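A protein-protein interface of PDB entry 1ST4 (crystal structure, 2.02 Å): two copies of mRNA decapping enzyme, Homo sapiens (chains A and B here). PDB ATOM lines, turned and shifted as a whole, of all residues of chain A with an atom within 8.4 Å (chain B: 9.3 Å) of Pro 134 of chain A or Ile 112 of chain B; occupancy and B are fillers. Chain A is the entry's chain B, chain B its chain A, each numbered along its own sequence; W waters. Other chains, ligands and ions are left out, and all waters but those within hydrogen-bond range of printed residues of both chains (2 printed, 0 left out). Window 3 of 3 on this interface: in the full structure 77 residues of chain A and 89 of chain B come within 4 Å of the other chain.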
ATOM      1  N   PRO A  43      15.253  26.623  15.449  1.00  0.00           N
ATOM      2  CA  PRO A  43      14.792  25.235  15.506  1.00  0.00           C
ATOM      3  C   PRO A  43      14.028  24.704  14.287  1.00  0.00           C
ATOM      4  O   PRO A  43      13.569  23.559  14.431  1.00  0.00           O
ATOM      5  CB  PRO A  43      13.900  25.202  16.743  1.00  0.00           C
ATOM      6  CG  PRO A  43      13.542  26.537  16.964  1.00  0.00           C
ATOM      7  CD  PRO A  43      14.661  27.434  16.515  1.00  0.00           C
ATOM      8  N   PHE A  44      13.869  25.466  13.195  1.00  0.00           N
ATOM      9  CA  PHE A  44      13.211  24.982  12.007  1.00  0.00           C
ATOM     10  C   PHE A  44      13.836  25.578  10.763  1.00  0.00           C
ATOM     11  O   PHE A  44      14.707  26.442  10.865  1.00  0.00           O
ATOM     12  CB  PHE A  44      11.738  25.373  12.045  1.00  0.00           C
ATOM     13  CG  PHE A  44      11.501  26.877  12.374  1.00  0.00           C
ATOM     14  CD1 PHE A  44      11.762  27.886  11.418  1.00  0.00           C
ATOM     15  CD2 PHE A  44      11.034  27.248  13.618  1.00  0.00           C
ATOM     16  CE1 PHE A  44      11.568  29.238  11.715  1.00  0.00           C
ATOM     17  CE2 PHE A  44      10.799  28.637  13.924  1.00  0.00           C
ATOM     18  CZ  PHE A  44      11.057  29.607  12.974  1.00  0.00           C
ATOM     19  N   VAL A  68       6.325  26.657   9.206  1.00  0.00           N
ATOM     20  CA  VAL A  68       7.751  26.309   9.042  1.00  0.00           C
ATOM     21  C   VAL A  68       7.962  24.893   8.438  1.00  0.00           C
ATOM     22  O   VAL A  68       7.004  24.121   8.371  1.00  0.00           O
ATOM     23  CB  VAL A  68       8.453  26.503  10.410  1.00  0.00           C
ATOM     24  CG1 VAL A  68       8.376  28.028  10.798  1.00  0.00           C
ATOM     25  CG2 VAL A  68       7.792  25.659  11.516  1.00  0.00           C
ATOM     26  N   ASN A  69       9.170  24.556   7.942  1.00  0.00           N
ATOM     27  CA  ASN A  69       9.522  23.155   7.468  1.00  0.00           C
ATOM     28  C   ASN A  69       8.794  22.615   6.169  1.00  0.00           C
ATOM     29  O   ASN A  69       8.967  21.423   5.793  1.00  0.00           O
ATOM     30  CB  ASN A  69       9.373  22.085   8.579  1.00  0.00           C
ATOM     31  CG  ASN A  69      10.322  22.313   9.787  1.00  0.00           C
ATOM     32  OD1 ASN A  69      11.442  22.839   9.630  1.00  0.00           O
ATOM     33  ND2 ASN A  69       9.866  21.906  11.001  1.00  0.00           N
ATOM     34  N   GLY A  77       4.197  21.101   6.716  1.00  0.00           N
ATOM     35  CA  GLY A  77       4.643  22.210   7.549  1.00  0.00           C
ATOM     36  C   GLY A  77       4.100  22.240   8.968  1.00  0.00           C
ATOM     37  O   GLY A  77       3.020  21.703   9.210  1.00  0.00           O
ATOM     38  N   GLU A  78       4.821  22.879   9.888  1.00  0.00           N
ATOM     39  CA  GLU A  78       4.342  23.089  11.272  1.00  0.00           C
ATOM     40  C   GLU A  78       4.129  24.595  11.629  1.00  0.00           C
ATOM     41  O   GLU A  78       4.573  25.496  10.879  1.00  0.00           O
ATOM     42  CB  GLU A  78       5.323  22.467  12.277  1.00  0.00           C
ATOM     43  CG  GLU A  78       5.592  20.971  12.022  1.00  0.00           C
ATOM     44  CD  GLU A  78       6.750  20.443  12.867  1.00  0.00           C
ATOM     45  OE1 GLU A  78       6.522  19.973  14.015  1.00  0.00           O
ATOM     46  OE2 GLU A  78       7.911  20.517  12.385  1.00  0.00           O
ATOM     47  N   ASP A  79       3.555  24.812  12.803  1.00  0.00           N
ATOM     48  CA  ASP A  79       3.283  26.109  13.368  1.00  0.00           C
ATOM     49  C   ASP A  79       4.426  26.610  14.283  1.00  0.00           C
ATOM     50  O   ASP A  79       4.854  25.883  15.219  1.00  0.00           O
ATOM     51  CB  ASP A  79       2.002  26.094  14.214  1.00  0.00           C
ATOM     52  CG  ASP A  79       0.742  25.776  13.398  1.00  0.00           C
ATOM     53  OD1 ASP A  79       0.560  26.374  12.287  1.00  0.00           O
ATOM     54  OD2 ASP A  79      -0.112  24.921  13.818  1.00  0.00           O
ATOM     55  N   ALA A  80       4.841  27.877  14.089  1.00  0.00           N
ATOM     56  CA  ALA A  80       5.795  28.538  15.005  1.00  0.00           C
ATOM     57  C   ALA A  80       5.272  29.973  15.337  1.00  0.00           C
ATOM     58  O   ALA A  80       4.708  30.611  14.409  1.00  0.00           O
ATOM     59  CB  ALA A  80       7.108  28.605  14.369  1.00  0.00           C
ATOM     60  N   VAL A  81       5.431  30.450  16.605  1.00  0.00           N
ATOM     61  CA  VAL A  81       5.360  31.884  16.852  1.00  0.00           C
ATOM     62  C   VAL A  81       6.775  32.470  16.951  1.00  0.00           C
ATOM     63  O   VAL A  81       7.637  31.842  17.596  1.00  0.00           O
ATOM     64  CB  VAL A  81       4.595  32.217  18.160  1.00  0.00           C
ATOM     65  CG1 VAL A  81       4.686  33.679  18.449  1.00  0.00           C
ATOM     66  CG2 VAL A  81       3.160  31.847  17.985  1.00  0.00           C
ATOM     67  N   THR A 130      12.188  35.774  20.075  1.00  0.00           N
ATOM     68  CA  THR A 130      11.678  34.710  20.939  1.00  0.00           C
ATOM     69  C   THR A 130      10.940  33.763  19.998  1.00  0.00           C
ATOM     70  O   THR A 130      10.119  34.219  19.155  1.00  0.00           O
ATOM     71  CB  THR A 130      10.742  35.239  22.011  1.00  0.00           C
ATOM     72  OG1 THR A 130      11.420  36.174  22.864  1.00  0.00           O
ATOM     73  CG2 THR A 130      10.198  34.126  22.953  1.00  0.00           C
ATOM     74  N   VAL A 131      11.210  32.459  20.103  1.00  0.00           N
ATOM     75  CA  VAL A 131      10.545  31.478  19.236  1.00  0.00           C
ATOM     76  C   VAL A 131       9.677  30.468  19.999  1.00  0.00           C
ATOM     77  O   VAL A 131      10.144  29.905  20.950  1.00  0.00           O
ATOM     78  CB  VAL A 131      11.606  30.690  18.397  1.00  0.00           C
ATOM     79  CG1 VAL A 131      10.954  29.672  17.465  1.00  0.00           C
ATOM     80  CG2 VAL A 131      12.459  31.581  17.719  1.00  0.00           C
ATOM     81  N   VAL A 132       8.406  30.267  19.638  1.00  0.00           N
ATOM     82  CA  VAL A 132       7.644  29.126  20.179  1.00  0.00           C
ATOM     83  C   VAL A 132       7.477  28.056  19.100  1.00  0.00           C
ATOM     84  O   VAL A 132       6.816  28.318  18.052  1.00  0.00           O
ATOM     85  CB  VAL A 132       6.256  29.495  20.643  1.00  0.00           C
ATOM     86  CG1 VAL A 132       5.597  28.303  21.237  1.00  0.00           C
ATOM     87  CG2 VAL A 132       6.322  30.597  21.727  1.00  0.00           C
ATOM     88  N   TYR A 133       8.142  26.897  19.280  1.00  0.00           N
ATOM     89  CA  TYR A 133       8.119  25.856  18.240  1.00  0.00           C
ATOM     90  C   TYR A 133       8.218  24.437  18.871  1.00  0.00           C
ATOM     91  O   TYR A 133       9.205  24.168  19.545  1.00  0.00           O
ATOM     92  CB  TYR A 133       9.268  25.988  17.220  1.00  0.00           C
ATOM     93  CG  TYR A 133       9.441  24.754  16.337  1.00  0.00           C
ATOM     94  CD1 TYR A 133       8.569  24.513  15.236  1.00  0.00           C
ATOM     95  CD2 TYR A 133      10.458  23.788  16.634  1.00  0.00           C
ATOM     96  CE1 TYR A 133       8.700  23.383  14.444  1.00  0.00           C
ATOM     97  CE2 TYR A 133      10.605  22.626  15.880  1.00  0.00           C
ATOM     98  CZ  TYR A 133       9.739  22.423  14.777  1.00  0.00           C
ATOM     99  OH  TYR A 133       9.904  21.286  14.023  1.00  0.00           O
ATOM    100  N   PRO A 134       7.244  23.555  18.574  1.00  0.00           N
ATOM    101  CA  PRO A 134       6.104  23.906  17.688  1.00  0.00           C
ATOM    102  C   PRO A 134       5.006  24.613  18.459  1.00  0.00           C
ATOM    103  O   PRO A 134       4.907  24.366  19.640  1.00  0.00           O
ATOM    104  CB  PRO A 134       5.613  22.531  17.163  1.00  0.00           C
ATOM    105  CG  PRO A 134       6.152  21.465  18.219  1.00  0.00           C
ATOM    106  CD  PRO A 134       7.206  22.142  19.045  1.00  0.00           C
ATOM    107  N   ALA A 135       4.230  25.515  17.843  1.00  0.00           N
ATOM    108  CA  ALA A 135       3.258  26.274  18.654  1.00  0.00           C
ATOM    109  C   ALA A 135       1.869  25.667  18.455  1.00  0.00           C
ATOM    110  O   ALA A 135       1.617  25.080  17.409  1.00  0.00           O
ATOM    111  CB  ALA A 135       3.234  27.771  18.264  1.00  0.00           C
ATOM    112  N   THR A 136       1.004  25.836  19.453  1.00  0.00           N
ATOM    113  CA  THR A 136      -0.359  25.284  19.432  1.00  0.00           C
ATOM    114  C   THR A 136      -1.312  26.424  19.339  1.00  0.00           C
ATOM    115  O   THR A 136      -0.956  27.580  19.604  1.00  0.00           O
ATOM    116  CB  THR A 136      -0.702  24.531  20.718  1.00  0.00           C
ATOM    117  OG1 THR A 136      -0.641  25.416  21.848  1.00  0.00           O
ATOM    118  CG2 THR A 136       0.366  23.461  21.025  1.00  0.00           C
ATOM    119  N   GLU A 137      -2.555  26.069  19.006  1.00  0.00           N
ATOM    120  CA  GLU A 137      -3.645  27.002  18.903  1.00  0.00           C
ATOM    121  C   GLU A 137      -3.786  27.847  20.199  1.00  0.00           C
ATOM    122  O   GLU A 137      -4.235  29.010  20.133  1.00  0.00           O
ATOM    123  CB  GLU A 137      -4.909  26.245  18.433  1.00  0.00           C
ATOM    124  CG  GLU A 137      -6.226  27.018  18.506  1.00  0.00           C
ATOM    125  CD  GLU A 137      -6.347  28.194  17.500  1.00  0.00           C
ATOM    126  OE1 GLU A 137      -7.023  29.177  17.907  1.00  0.00           O
ATOM    127  OE2 GLU A 137      -5.794  28.152  16.343  1.00  0.00           O
ATOM    128  N   HIS A 139      -1.124  28.894  21.864  1.00  0.00           N
ATOM    129  CA  HIS A 139      -0.103  29.927  21.763  1.00  0.00           C
ATOM    130  C   HIS A 139      -0.673  31.006  20.846  1.00  0.00           C
ATOM    131  O   HIS A 139      -0.608  32.181  21.189  1.00  0.00           O
ATOM    132  CB  HIS A 139       1.241  29.364  21.276  1.00  0.00           C
ATOM    133  CG  HIS A 139       1.880  28.406  22.241  1.00  0.00           C
ATOM    134  ND1 HIS A 139       2.151  27.091  21.910  1.00  0.00           N
ATOM    135  CD2 HIS A 139       2.288  28.565  23.529  1.00  0.00           C
ATOM    136  CE1 HIS A 139       2.690  26.479  22.952  1.00  0.00           C
ATOM    137  NE2 HIS A 139       2.795  27.354  23.944  1.00  0.00           N
ATOM    138  N   LEU A 140      -1.297  30.612  19.736  1.00  0.00           N
ATOM    139  CA  LEU A 140      -1.887  31.614  18.848  1.00  0.00           C
ATOM    140  C   LEU A 140      -2.870  32.535  19.536  1.00  0.00           C
ATOM    141  O   LEU A 140      -2.723  33.758  19.464  1.00  0.00           O
ATOM    142  CB  LEU A 140      -2.465  30.997  17.614  1.00  0.00           C
ATOM    143  CG  LEU A 140      -1.538  29.947  17.059  1.00  0.00           C
ATOM    144  CD1 LEU A 140      -2.298  28.945  16.163  1.00  0.00           C
ATOM    145  CD2 LEU A 140      -0.361  30.577  16.336  1.00  0.00           C
ATOM    146  N   PHE B 108      18.336  31.693  25.720  1.00  0.00           N
ATOM    147  CA  PHE B 108      17.554  30.729  26.598  1.00  0.00           C
ATOM    148  C   PHE B 108      16.954  29.615  25.750  1.00  0.00           C
ATOM    149  O   PHE B 108      16.468  29.863  24.631  1.00  0.00           O
ATOM    150  CB  PHE B 108      16.282  31.230  27.295  1.00  0.00           C
ATOM    151  CG  PHE B 108      16.394  32.562  27.996  1.00  0.00           C
ATOM    152  CD1 PHE B 108      15.411  33.589  27.725  1.00  0.00           C
ATOM    153  CD2 PHE B 108      17.400  32.800  28.952  1.00  0.00           C
ATOM    154  CE1 PHE B 108      15.451  34.818  28.323  1.00  0.00           C
ATOM    155  CE2 PHE B 108      17.446  34.041  29.585  1.00  0.00           C
ATOM    156  CZ  PHE B 108      16.461  35.071  29.263  1.00  0.00           C
ATOM    157  N   SER B 109      16.900  28.414  26.319  1.00  0.00           N
ATOM    158  CA  SER B 109      16.490  27.216  25.596  1.00  0.00           C
ATOM    159  C   SER B 109      15.668  26.403  26.584  1.00  0.00           C
ATOM    160  O   SER B 109      16.112  26.146  27.700  1.00  0.00           O
ATOM    161  CB  SER B 109      17.736  26.398  25.149  1.00  0.00           C
ATOM    162  OG  SER B 109      17.481  25.518  24.053  1.00  0.00           O
ATOM    163  N   ASN B 110      14.455  26.033  26.200  1.00  0.00           N
ATOM    164  CA  ASN B 110      13.747  24.967  26.911  1.00  0.00           C
ATOM    165  C   ASN B 110      12.570  24.435  26.135  1.00  0.00           C
ATOM    166  O   ASN B 110      11.531  25.120  25.998  1.00  0.00           O
ATOM    167  CB  ASN B 110      13.312  25.310  28.369  1.00  0.00           C
ATOM    168  CG  ASN B 110      13.434  24.071  29.346  1.00  0.00           C
ATOM    169  OD1 ASN B 110      12.646  23.076  29.278  1.00  0.00           O
ATOM    170  ND2 ASN B 110      14.423  24.131  30.234  1.00  0.00           N
ATOM    171  N   ASP B 111      12.753  23.176  25.700  1.00  0.00           N
ATOM    172  CA  ASP B 111      11.690  22.363  25.096  1.00  0.00           C
ATOM    173  C   ASP B 111      11.212  23.074  23.807  1.00  0.00           C
ATOM    174  O   ASP B 111      11.935  22.994  22.804  1.00  0.00           O
ATOM    175  CB  ASP B 111      10.556  22.054  26.105  1.00  0.00           C
ATOM    176  CG  ASP B 111       9.578  20.977  25.591  1.00  0.00           C
ATOM    177  OD1 ASP B 111       9.994  19.986  24.914  1.00  0.00           O
ATOM    178  OD2 ASP B 111       8.339  21.041  25.825  1.00  0.00           O
ATOM    179  N   ILE B 112      10.067  23.802  23.864  1.00  0.00           N
ATOM    180  CA  ILE B 112       9.509  24.602  22.729  1.00  0.00           C
ATOM    181  C   ILE B 112       9.805  26.153  22.745  1.00  0.00           C
ATOM    182  O   ILE B 112       9.821  26.773  21.706  1.00  0.00           O
ATOM    183  CB  ILE B 112       7.975  24.291  22.492  1.00  0.00           C
ATOM    184  CG1 ILE B 112       7.066  25.070  23.454  1.00  0.00           C
ATOM    185  CG2 ILE B 112       7.712  22.794  22.633  1.00  0.00           C
ATOM    186  CD1 ILE B 112       5.592  25.000  23.056  1.00  0.00           C
ATOM    187  N   TYR B 113      10.025  26.748  23.909  1.00  0.00           N
ATOM    188  CA  TYR B 113      10.506  28.128  24.047  1.00  0.00           C
ATOM    189  C   TYR B 113      12.050  28.312  23.859  1.00  0.00           C
ATOM    190  O   TYR B 113      12.833  27.360  24.111  1.00  0.00           O
ATOM    191  CB  TYR B 113      10.081  28.623  25.423  1.00  0.00           C
ATOM    192  CG  TYR B 113       8.666  28.146  25.721  1.00  0.00           C
ATOM    193  CD1 TYR B 113       8.419  26.885  26.420  1.00  0.00           C
ATOM    194  CD2 TYR B 113       7.559  28.918  25.277  1.00  0.00           C
ATOM    195  CE1 TYR B 113       7.078  26.455  26.671  1.00  0.00           C
ATOM    196  CE2 TYR B 113       6.250  28.501  25.489  1.00  0.00           C
ATOM    197  CZ  TYR B 113       5.995  27.280  26.194  1.00  0.00           C
ATOM    198  OH  TYR B 113       4.656  26.935  26.377  1.00  0.00           O
ATOM    199  N   SER B 114      12.460  29.508  23.403  1.00  0.00           N
ATOM    200  CA  SER B 114      13.885  29.902  23.200  1.00  0.00           C
ATOM    201  C   SER B 114      13.981  31.365  22.713  1.00  0.00           C
ATOM    202  O   SER B 114      13.093  31.848  22.025  1.00  0.00           O
ATOM    203  CB  SER B 114      14.646  28.953  22.264  1.00  0.00           C
ATOM    204  OG  SER B 114      13.927  28.699  21.086  1.00  0.00           O
ATOM    205  N   THR B 115      15.028  32.053  23.135  1.00  0.00           N
ATOM    206  CA  THR B 115      15.294  33.457  22.913  1.00  0.00           C
ATOM    207  C   THR B 115      16.678  33.555  22.356  1.00  0.00           C
ATOM    208  O   THR B 115      17.633  32.934  22.932  1.00  0.00           O
ATOM    209  CB  THR B 115      15.202  34.188  24.214  1.00  0.00           C
ATOM    210  OG1 THR B 115      13.895  33.961  24.775  1.00  0.00           O
ATOM    211  CG2 THR B 115      15.266  35.783  24.038  1.00  0.00           C
ATOM    212  N   TYR B 116      16.792  34.261  21.223  1.00  0.00           N
ATOM    213  CA  TYR B 116      18.045  34.493  20.561  1.00  0.00           C
ATOM    214  C   TYR B 116      18.342  35.980  20.546  1.00  0.00           C
ATOM    215  O   TYR B 116      17.438  36.791  20.898  1.00  0.00           O
ATOM    216  CB  TYR B 116      17.951  34.028  19.106  1.00  0.00           C
ATOM    217  CG  TYR B 116      17.603  32.552  18.956  1.00  0.00           C
ATOM    218  CD1 TYR B 116      16.289  32.101  19.159  1.00  0.00           C
ATOM    219  CD2 TYR B 116      18.617  31.593  18.689  1.00  0.00           C
ATOM    220  CE1 TYR B 116      15.940  30.798  19.031  1.00  0.00           C
ATOM    221  CE2 TYR B 116      18.265  30.223  18.609  1.00  0.00           C
ATOM    222  CZ  TYR B 116      16.940  29.853  18.757  1.00  0.00           C
ATOM    223  OH  TYR B 116      16.583  28.555  18.634  1.00  0.00           O
HETATM  224  O   HOH W   1      11.687  36.196  25.556  1.00  0.00           O
HETATM  225  O   HOH W   2      12.018  27.285  20.362  1.00  0.00           O
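No position is printed for both chains.
The side-chain amide nitrogen (ND2) of Asn 69 of chain A is in hydrogen-bond range of the side-chain hydroxyl (OH) of Tyr 133 of chain A, 3.1 Å away.
OH of Tyr 133 of chain A lies within hydrogen-bond range of OE2 of Glu 78 of chain A.
O of Val 81 of chain A lies within hydrogen-bond range of N of Val 132 of chain A, 2.7 Å away.
The backbone carbonyl oxygen (O) of Phe 108 of chain B sits at hydrogen-bond distance from the backbone NH (N) of Thr 115 of chain B.
The backbone NH (N) of Thr 136 of chain A is in hydrogen-bond range of a ring nitrogen (ND1) of His 139 of chain A, 3.0 Å away.
The backbone NH (N) of Val 131 of chain A is in hydrogen-bond range of the backbone carbonyl oxygen (O) of Ser 114 of chain B.
The backbone carbonyl oxygen of Ile 112 of chain B sits close to the backbone carbonyl oxygen of Val 131 of chain A (3.2 Å).
The side-chain hydroxyl (OH) of Tyr 113 of chain B sits at hydrogen-bond distance from a ring nitrogen (NE2) of His 139 of chain A, 3.1 Å away.
The backbone NH of Tyr 133 of chain A sits at hydrogen-bond distance from the backbone carbonyl oxygen of Ile 112 of chain B (3.0 Å).
OH of Tyr 116 of chain B touches CD of Pro 43 of chain A, at 3.1 Å.
Thr 130 of chain A touches Ser 114 of chain B.
Thr 115 of chain B touches Thr 130 of chain A (OG1 to OG1, 3.8 Å).
Tyr 113 of chain B touches Val 131 of chain A (CA to O, 3.6 Å).
Val 131 of chain A touches Tyr 116 of chain B.
Ile 112 of chain B touches Val 132 of chain A.
CD1 of Ile 112 of chain B touches O of Pro 134 of chain A, at 3.5 Å.
Ile 112 of chain B touches His 139 of chain A (CD1 to CE1, 3.3 Å).
Printed residues of chain B that touch a printed residue of chain A: Ile 112, Tyr 113, Ser 114, Thr 115 and Tyr 116.
Hydrophobic or aromatic side chains of chain B that line the printed part of chain A: Ile 112, Tyr 113 and Tyr 116.
Among the printed residues, no Asp or Glu carboxylate lies within 4 Å of a Lys or Arg side-chain nitrogen of the other chain.
Water W2 lies within hydrogen-bond range of OG of Ser 114 of chain B (2.5 Å), O of Ile 112 of chain B (2.6 Å) and O of Val 131 of chain A (3.3 Å).
Water W1 lies within hydrogen-bond range of OG1 of Thr 130 of chain A (2.7 Å) and OG1 of Thr 115 of chain B (3.2 Å).
Asn 69 of chain A touches none of the printed residues of chain B.
Gly 77 of chain A touches none of the printed residues of chain B.
Printed residues of chain B within 4 Å of Thr 130 of chain A: Ser 114 (3.4 Å) and Thr 115 (3.8 Å).
Of the printed residues of chain B, Val 131 of chain A touches Ile 112 (3.2 Å), Tyr 113 (3.6 Å), Ser 114 (2.8 Å) and Tyr 116 (3.8 Å).
Of the printed residues of chain B, Tyr 133 of chain A touches Ile 112 (3.0 Å).
Pro 134 of chain A touches one residue of chain B.
Of the printed residues of chain B, His 139 of chain A touches Ile 112 and Tyr 113.
Of the printed residues of chain A, Ile 112 of chain B touches Val 131, Val 132, Tyr 133, Pro 134 and His 139.
Of chain A, only Val 131 and His 139 come within 4 Å of Tyr 113 of chain B.
Printed residues of chain A within 4 Å of Thr 115 of chain B: Thr 130.
The nearest residue of chain A that does not touch Ile 112 of chain B is Ala 135 of chain A (5.1 Å).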
